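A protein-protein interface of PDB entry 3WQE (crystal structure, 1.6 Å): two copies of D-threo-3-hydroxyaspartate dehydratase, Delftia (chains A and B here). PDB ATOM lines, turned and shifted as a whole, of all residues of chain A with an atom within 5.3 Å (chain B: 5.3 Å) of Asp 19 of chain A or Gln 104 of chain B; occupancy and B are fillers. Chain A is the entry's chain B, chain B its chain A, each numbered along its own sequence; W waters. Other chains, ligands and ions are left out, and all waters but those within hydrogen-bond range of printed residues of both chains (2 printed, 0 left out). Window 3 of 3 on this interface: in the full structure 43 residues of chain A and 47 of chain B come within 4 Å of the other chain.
No position is printed for both chains. Of the 7 pairs that touch across the chains among the printed residues, none has its exchanged pair printed and touching as well.
Thr 20 of chain A touches His 100 of chain B (OG1 to CE1, 3.5 Å). Pro 21 of chain A touches Trp 390 of chain B (CG to CE2, 3.4 Å). His 100 of chain B touches Arg 354 of chain A.
The guanidinium group (NH1) of Arg 101 of chain B sits at hydrogen-bond distance from a ring nitrogen (NE2) of His 100 of chain B (3.3 Å). The backbone carbonyl oxygen of Leu 18 of chain A sits at hydrogen-bond distance from the guanidinium group of Arg 354 of chain A (2.8 Å).
The side-chain carboxylate of Asp 19 of chain A sits close to the side-chain amide oxygen of Gln 104 of chain B (3.3 Å). The side-chain carboxylate (OD1) of Asp 19 of chain A lies within salt-bridge range of the guanidinium group (NH1) of Arg 101 of chain B. The side-chain carboxylate of Asp 19 of chain A is in hydrogen-bond range of a ring nitrogen (NE2) of His 100 of chain B. The guanidinium group (NH1) of Arg 101 of chain B sits at hydrogen-bond distance from the backbone carbonyl oxygen (O) of Thr 20 of chain A (2.9 Å).
Of the 8 printed residues of chain A, 4 touch a printed residue of chain B. Printed residues of chain A that touch a printed residue of chain B: Asp 19, Thr 20, Pro 21 and Arg 354. Hydrophobic or aromatic side chains of chain A within 4 Å of the printed part of chain B: Pro 21. Printed residues of chain B that touch a printed residue of chain A: His 100, Arg 101, Gln 104 and Trp 390. Among the printed residues, 7 pairs touch across the chains. Among the printed residues, Asp or Glu carboxylates within 4 Å of a Lys or Arg side-chain nitrogen of the other chain: Asp 19 of chain A with Arg 101 of chain B.
Water W2 bridges OD2 of Asp 19 of chain A (2.7 Å) and OXT of Trp 390 of chain B (2.7 Å). Water W1 lies within hydrogen-bond range of O of Thr 20 of chain A (2.9 Å) and NH1 of Arg 101 of chain B (3.3 Å).
Printed residues of chain B within 4 Å of Asp 19 of chain A: His 100, Arg 101 and Gln 104. Of the printed residues of chain A, Gln 104 of chain B touches Asp 19. Printed residues of chain B within 4 Å of Pro 21 of chain A: Trp 390 (3.4 Å). Printed residues of chain B within 4 Å of Thr 20 of chain A: His 100 (3.5 Å) and Arg 101 (2.9 Å). Of the printed residues of chain B, Arg 354 of chain A touches His 100 (3.6 Å). Of the printed residues of chain A, Trp 390 of chain B touches Pro 21 (3.4 Å). Arg 109 of chain B touches none of the printed residues of chain A. The nearest printed residue of chain B that does not touch Asp 19 of chain A is Trp 390 of chain B (4.3 Å).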
ATOM      1  N   THR A  17      22.555  -9.283 -14.991  1.00  0.00           N
ATOM      2  CA  THR A  17      21.752 -10.466 -15.154  1.00  0.00           C
ATOM      3  C   THR A  17      21.589 -10.768 -16.654  1.00  0.00           C
ATOM      4  O   THR A  17      21.302 -11.936 -16.953  1.00  0.00           O
ATOM      5  CB  THR A  17      20.334 -10.372 -14.539  1.00  0.00           C
ATOM      6  OG1 THR A  17      19.571  -9.396 -15.266  1.00  0.00           O
ATOM      7  CG2 THR A  17      20.435 -10.124 -13.005  1.00  0.00           C
ATOM      8  N   LEU A  18      21.835  -9.827 -17.567  1.00  0.00           N
ATOM      9  CA  LEU A  18      21.778 -10.110 -19.002  1.00  0.00           C
ATOM     10  C   LEU A  18      22.797 -11.192 -19.372  1.00  0.00           C
ATOM     11  O   LEU A  18      23.894 -11.234 -18.857  1.00  0.00           O
ATOM     12  CB  LEU A  18      22.175  -8.857 -19.819  1.00  0.00           C
ATOM     13  CG  LEU A  18      21.104  -7.767 -19.840  1.00  0.00           C
ATOM     14  CD1 LEU A  18      21.689  -6.555 -20.562  1.00  0.00           C
ATOM     15  CD2 LEU A  18      19.796  -8.233 -20.580  1.00  0.00           C
ATOM     16  N   ASP A  19      22.463 -12.005 -20.363  1.00  0.00           N
ATOM     17  CA  ASP A  19      23.497 -12.871 -20.943  1.00  0.00           C
ATOM     18  C   ASP A  19      24.337 -11.940 -21.853  1.00  0.00           C
ATOM     19  O   ASP A  19      23.897 -10.851 -22.266  1.00  0.00           O
ATOM     20  CB  ASP A  19      22.888 -13.951 -21.858  1.00  0.00           C
ATOM     21  CG  ASP A  19      23.948 -15.066 -22.263  1.00  0.00           C
ATOM     22  OD1 ASP A  19      25.065 -15.145 -21.628  1.00  0.00           O
ATOM     23  OD2 ASP A  19      23.648 -15.828 -23.273  1.00  0.00           O
ATOM     24  N   THR A  20      25.592 -12.341 -22.051  1.00  0.00           N
ATOM     25  CA  THR A  20      26.497 -11.581 -22.928  1.00  0.00           C
ATOM     26  C   THR A  20      26.863 -12.403 -24.163  1.00  0.00           C
ATOM     27  O   THR A  20      26.820 -13.668 -24.090  1.00  0.00           O
ATOM     28  CB  THR A  20      27.804 -11.254 -22.115  1.00  0.00           C
ATOM     29  OG1 THR A  20      28.315 -12.450 -21.546  1.00  0.00           O
ATOM     30  CG2 THR A  20      27.508 -10.232 -20.985  1.00  0.00           C
ATOM     31  N   PRO A  21      27.237 -11.784 -25.233  1.00  0.00           N
ATOM     32  CA  PRO A  21      27.304 -10.340 -25.388  1.00  0.00           C
ATOM     33  C   PRO A  21      25.899  -9.726 -25.593  1.00  0.00           C
ATOM     34  O   PRO A  21      24.950 -10.359 -26.029  1.00  0.00           O
ATOM     35  CB  PRO A  21      28.129 -10.174 -26.673  1.00  0.00           C
ATOM     36  CG  PRO A  21      27.689 -11.354 -27.536  1.00  0.00           C
ATOM     37  CD  PRO A  21      27.614 -12.492 -26.510  1.00  0.00           C
ATOM     38  N   ALA A  22      25.802  -8.437 -25.290  1.00  0.00           N
ATOM     39  CA  ALA A  22      24.539  -7.630 -25.503  1.00  0.00           C
ATOM     40  C   ALA A  22      24.870  -6.227 -25.933  1.00  0.00           C
ATOM     41  O   ALA A  22      25.848  -5.672 -25.460  1.00  0.00           O
ATOM     42  CB  ALA A  22      23.745  -7.624 -24.146  1.00  0.00           C
ATOM     43  N   LEU A 271      28.186  -5.266 -23.993  1.00  0.00           N
ATOM     44  CA  LEU A 271      28.436  -5.901 -22.684  1.00  0.00           C
ATOM     45  C   LEU A 271      29.029  -7.276 -22.954  1.00  0.00           C
ATOM     46  O   LEU A 271      28.512  -8.025 -23.743  1.00  0.00           O
ATOM     47  CB  LEU A 271      27.075  -6.096 -21.995  1.00  0.00           C
ATOM     48  CG  LEU A 271      27.147  -6.592 -20.509  1.00  0.00           C
ATOM     49  CD1 LEU A 271      27.770  -5.516 -19.600  1.00  0.00           C
ATOM     50  CD2 LEU A 271      25.726  -6.939 -20.079  1.00  0.00           C
ATOM     51  N   ARG A 354      32.541  -8.531 -16.027  1.00  0.00           N
ATOM     52  CA  ARG A 354      31.788  -7.949 -17.133  1.00  0.00           C
ATOM     53  C   ARG A 354      32.375  -6.618 -17.463  1.00  0.00           C
ATOM     54  O   ARG A 354      32.723  -5.776 -16.577  1.00  0.00           O
ATOM     55  CB  ARG A 354      30.330  -7.729 -16.746  1.00  0.00           C
ATOM     56  CG  ARG A 354      29.597  -9.061 -16.624  1.00  0.00           C
ATOM     57  CD  ARG A 354      28.163  -9.011 -16.109  1.00  0.00           C
ATOM     58  NE  ARG A 354      27.625 -10.408 -16.256  1.00  0.00           N
ATOM     59  CZ  ARG A 354      26.572 -10.711 -17.001  1.00  0.00           C
ATOM     60  NH1 ARG A 354      25.694  -9.794 -17.346  1.00  0.00           N
ATOM     61  NH2 ARG A 354      26.279 -12.043 -17.154  1.00  0.00           N
ATOM     62  N   LEU B  77      25.283 -20.996 -27.130  1.00  0.00           N
ATOM     63  CA  LEU B  77      24.150 -21.850 -26.694  1.00  0.00           C
ATOM     64  C   LEU B  77      22.907 -21.584 -27.454  1.00  0.00           C
ATOM     65  O   LEU B  77      22.096 -22.504 -27.490  1.00  0.00           O
ATOM     66  CB  LEU B  77      23.980 -21.662 -25.172  1.00  0.00           C
ATOM     67  CG  LEU B  77      25.170 -22.246 -24.370  1.00  0.00           C
ATOM     68  CD1 LEU B  77      24.736 -22.120 -22.884  1.00  0.00           C
ATOM     69  CD2 LEU B  77      25.355 -23.784 -24.729  1.00  0.00           C
ATOM     70  N   GLU B  81      20.469 -24.560 -28.674  1.00  0.00           N
ATOM     71  CA  GLU B  81      18.989 -24.609 -28.569  1.00  0.00           C
ATOM     72  C   GLU B  81      18.306 -24.859 -29.936  1.00  0.00           C
ATOM     73  O   GLU B  81      17.406 -25.734 -29.997  1.00  0.00           O
ATOM     74  CB  GLU B  81      18.415 -23.250 -28.079  1.00  0.00           C
ATOM     75  CG  GLU B  81      18.914 -22.894 -26.704  1.00  0.00           C
ATOM     76  CD  GLU B  81      18.114 -23.522 -25.573  1.00  0.00           C
ATOM     77  OE1 GLU B  81      18.495 -23.271 -24.377  1.00  0.00           O
ATOM     78  OE2 GLU B  81      17.110 -24.265 -25.865  1.00  0.00           O
ATOM     79  N   HIS B 100      28.348 -18.121 -15.768  1.00  0.00           N
ATOM     80  CA  HIS B 100      27.015 -17.585 -15.709  1.00  0.00           C
ATOM     81  C   HIS B 100      26.098 -18.283 -16.692  1.00  0.00           C
ATOM     82  O   HIS B 100      24.898 -18.209 -16.477  1.00  0.00           O
ATOM     83  CB  HIS B 100      26.927 -16.042 -15.889  1.00  0.00           C
ATOM     84  CG  HIS B 100      27.075 -15.599 -17.255  1.00  0.00           C
ATOM     85  ND1 HIS B 100      28.275 -15.272 -17.789  1.00  0.00           N
ATOM     86  CD2 HIS B 100      26.142 -15.439 -18.266  1.00  0.00           C
ATOM     87  CE1 HIS B 100      28.090 -14.895 -19.093  1.00  0.00           C
ATOM     88  NE2 HIS B 100      26.784 -14.963 -19.375  1.00  0.00           N
ATOM     89  N   ARG B 101      26.644 -19.015 -17.649  1.00  0.00           N
ATOM     90  CA  ARG B 101      25.754 -19.720 -18.614  1.00  0.00           C
ATOM     91  C   ARG B 101      25.483 -21.129 -18.090  1.00  0.00           C
ATOM     92  O   ARG B 101      24.795 -21.883 -18.815  1.00  0.00           O
ATOM     93  CB  ARG B 101      26.436 -19.783 -19.987  1.00  0.00           C
ATOM     94  CG  ARG B 101      26.201 -18.447 -20.754  1.00  0.00           C
ATOM     95  CD  ARG B 101      26.652 -18.492 -22.251  1.00  0.00           C
ATOM     96  NE  ARG B 101      28.097 -18.174 -22.434  1.00  0.00           N
ATOM     97  CZ  ARG B 101      28.528 -16.900 -22.583  1.00  0.00           C
ATOM     98  NH1 ARG B 101      27.728 -15.840 -22.461  1.00  0.00           N
ATOM     99  NH2 ARG B 101      29.825 -16.698 -22.765  1.00  0.00           N
ATOM    100  N   LEU B 102      25.980 -21.503 -16.937  1.00  0.00           N
ATOM    101  CA  LEU B 102      25.747 -22.906 -16.454  1.00  0.00           C
ATOM    102  C   LEU B 102      24.248 -23.261 -16.305  1.00  0.00           C
ATOM    103  O   LEU B 102      23.909 -24.367 -16.620  1.00  0.00           O
ATOM    104  CB  LEU B 102      26.520 -23.183 -15.174  1.00  0.00           C
ATOM    105  CG  LEU B 102      27.999 -23.525 -15.429  1.00  0.00           C
ATOM    106  CD1 LEU B 102      28.827 -23.415 -14.165  1.00  0.00           C
ATOM    107  CD2 LEU B 102      28.184 -24.932 -16.066  1.00  0.00           C
ATOM    108  N   PRO B 103      23.394 -22.340 -15.834  1.00  0.00           N
ATOM    109  CA  PRO B 103      21.961 -22.762 -15.725  1.00  0.00           C
ATOM    110  C   PRO B 103      21.391 -23.108 -17.115  1.00  0.00           C
ATOM    111  O   PRO B 103      20.603 -24.054 -17.157  1.00  0.00           O
ATOM    112  CB  PRO B 103      21.251 -21.538 -15.078  1.00  0.00           C
ATOM    113  CG  PRO B 103      22.394 -20.942 -14.206  1.00  0.00           C
ATOM    114  CD  PRO B 103      23.665 -21.084 -15.016  1.00  0.00           C
ATOM    115  N   GLN B 104      21.809 -22.402 -18.175  1.00  0.00           N
ATOM    116  CA  GLN B 104      21.334 -22.628 -19.551  1.00  0.00           C
ATOM    117  C   GLN B 104      21.840 -24.010 -19.990  1.00  0.00           C
ATOM    118  O   GLN B 104      21.107 -24.813 -20.618  1.00  0.00           O
ATOM    119  CB  GLN B 104      21.873 -21.484 -20.473  1.00  0.00           C
ATOM    120  CG  GLN B 104      21.264 -20.055 -20.210  1.00  0.00           C
ATOM    121  CD  GLN B 104      22.108 -18.777 -20.754  1.00  0.00           C
ATOM    122  OE1 GLN B 104      22.395 -18.603 -21.945  1.00  0.00           O
ATOM    123  NE2 GLN B 104      22.374 -17.883 -19.881  1.00  0.00           N
ATOM    124  N   ALA B 105      23.094 -24.308 -19.724  1.00  0.00           N
ATOM    125  CA  ALA B 105      23.687 -25.574 -20.119  1.00  0.00           C
ATOM    126  C   ALA B 105      23.003 -26.697 -19.385  1.00  0.00           C
ATOM    127  O   ALA B 105      22.724 -27.775 -19.967  1.00  0.00           O
ATOM    128  CB  ALA B 105      25.203 -25.601 -19.830  1.00  0.00           C
ATOM    129  N   LEU B 106      22.765 -26.526 -18.081  1.00  0.00           N
ATOM    130  CA  LEU B 106      22.055 -27.557 -17.294  1.00  0.00           C
ATOM    131  C   LEU B 106      20.679 -27.847 -17.855  1.00  0.00           C
ATOM    132  O   LEU B 106      20.323 -29.078 -17.889  1.00  0.00           O
ATOM    133  CB  LEU B 106      21.891 -27.012 -15.851  1.00  0.00           C
ATOM    134  CG  LEU B 106      21.149 -27.926 -14.893  1.00  0.00           C
ATOM    135  CD1 LEU B 106      21.853 -29.285 -14.711  1.00  0.00           C
ATOM    136  CD2 LEU B 106      21.034 -27.285 -13.503  1.00  0.00           C
ATOM    137  N   GLN B 107      19.939 -26.815 -18.183  1.00  0.00           N
ATOM    138  CA  GLN B 107      18.542 -27.009 -18.625  1.00  0.00           C
ATOM    139  C   GLN B 107      18.577 -27.805 -19.998  1.00  0.00           C
ATOM    140  O   GLN B 107      17.777 -28.749 -20.153  1.00  0.00           O
ATOM    141  CB  GLN B 107      17.841 -25.667 -18.785  1.00  0.00           C
ATOM    142  CG  GLN B 107      16.372 -25.927 -19.068  1.00  0.00           C
ATOM    143  CD  GLN B 107      15.797 -25.061 -20.107  1.00  0.00           C
ATOM    144  OE1 GLN B 107      16.306 -25.010 -21.252  1.00  0.00           O
ATOM    145  NE2 GLN B 107      14.671 -24.407 -19.762  1.00  0.00           N
ATOM    146  N   LEU B 108      19.549 -27.509 -20.829  1.00  0.00           N
ATOM    147  CA  LEU B 108      19.711 -28.245 -22.142  1.00  0.00           C
ATOM    148  C   LEU B 108      20.010 -29.696 -21.833  1.00  0.00           C
ATOM    149  O   LEU B 108      19.377 -30.588 -22.444  1.00  0.00           O
ATOM    150  CB  LEU B 108      20.779 -27.658 -23.048  1.00  0.00           C
ATOM    151  CG  LEU B 108      20.284 -26.506 -23.830  1.00  0.00           C
ATOM    152  CD1 LEU B 108      21.541 -25.739 -24.331  1.00  0.00           C
ATOM    153  CD2 LEU B 108      19.462 -27.068 -25.071  1.00  0.00           C
ATOM    154  N   ARG B 109      20.944 -30.002 -20.915  1.00  0.00           N
ATOM    155  CA  ARG B 109      21.238 -31.422 -20.619  1.00  0.00           C
ATOM    156  C   ARG B 109      20.000 -32.082 -20.033  1.00  0.00           C
ATOM    157  O   ARG B 109      19.688 -33.263 -20.340  1.00  0.00           O
ATOM    158  CB  ARG B 109      22.457 -31.570 -19.632  1.00  0.00           C
ATOM    159  CG  ARG B 109      23.682 -31.172 -20.439  1.00  0.00           C
ATOM    160  CD  ARG B 109      24.956 -31.378 -19.554  1.00  0.00           C
ATOM    161  NE  ARG B 109      25.142 -32.764 -19.168  1.00  0.00           N
ATOM    162  CZ  ARG B 109      25.632 -33.770 -19.925  1.00  0.00           C
ATOM    163  NH1 ARG B 109      26.120 -33.572 -21.158  1.00  0.00           N
ATOM    164  NH2 ARG B 109      25.691 -34.946 -19.326  1.00  0.00           N
ATOM    165  N   TRP B 390      22.104 -14.233 -29.927  1.00  0.00           N
ATOM    166  CA  TRP B 390      22.583 -15.053 -28.837  1.00  0.00           C
ATOM    167  C   TRP B 390      21.421 -15.412 -27.965  1.00  0.00           C
ATOM    168  O   TRP B 390      20.284 -14.872 -28.074  1.00  0.00           O
ATOM    169  CB  TRP B 390      23.608 -14.275 -27.961  1.00  0.00           C
ATOM    170  CG  TRP B 390      24.864 -13.994 -28.721  1.00  0.00           C
ATOM    171  CD1 TRP B 390      26.046 -14.743 -28.752  1.00  0.00           C
ATOM    172  CD2 TRP B 390      25.090 -12.899 -29.632  1.00  0.00           C
ATOM    173  NE1 TRP B 390      26.919 -14.199 -29.574  1.00  0.00           N
ATOM    174  CE2 TRP B 390      26.428 -13.086 -30.181  1.00  0.00           C
ATOM    175  CE3 TRP B 390      24.306 -11.790 -30.099  1.00  0.00           C
ATOM    176  CZ2 TRP B 390      26.982 -12.218 -31.108  1.00  0.00           C
ATOM    177  CZ3 TRP B 390      24.914 -10.948 -31.064  1.00  0.00           C
ATOM    178  CH2 TRP B 390      26.194 -11.171 -31.591  1.00  0.00           C
ATOM    179  OXT TRP B 390      21.628 -16.283 -27.093  1.00  0.00           O
HETATM  180  O   HOH W   1      27.775 -15.843 -25.769  1.00  0.00           O
HETATM  181  O   HOH W   2      21.370 -15.370 -24.557  1.00  0.00           O
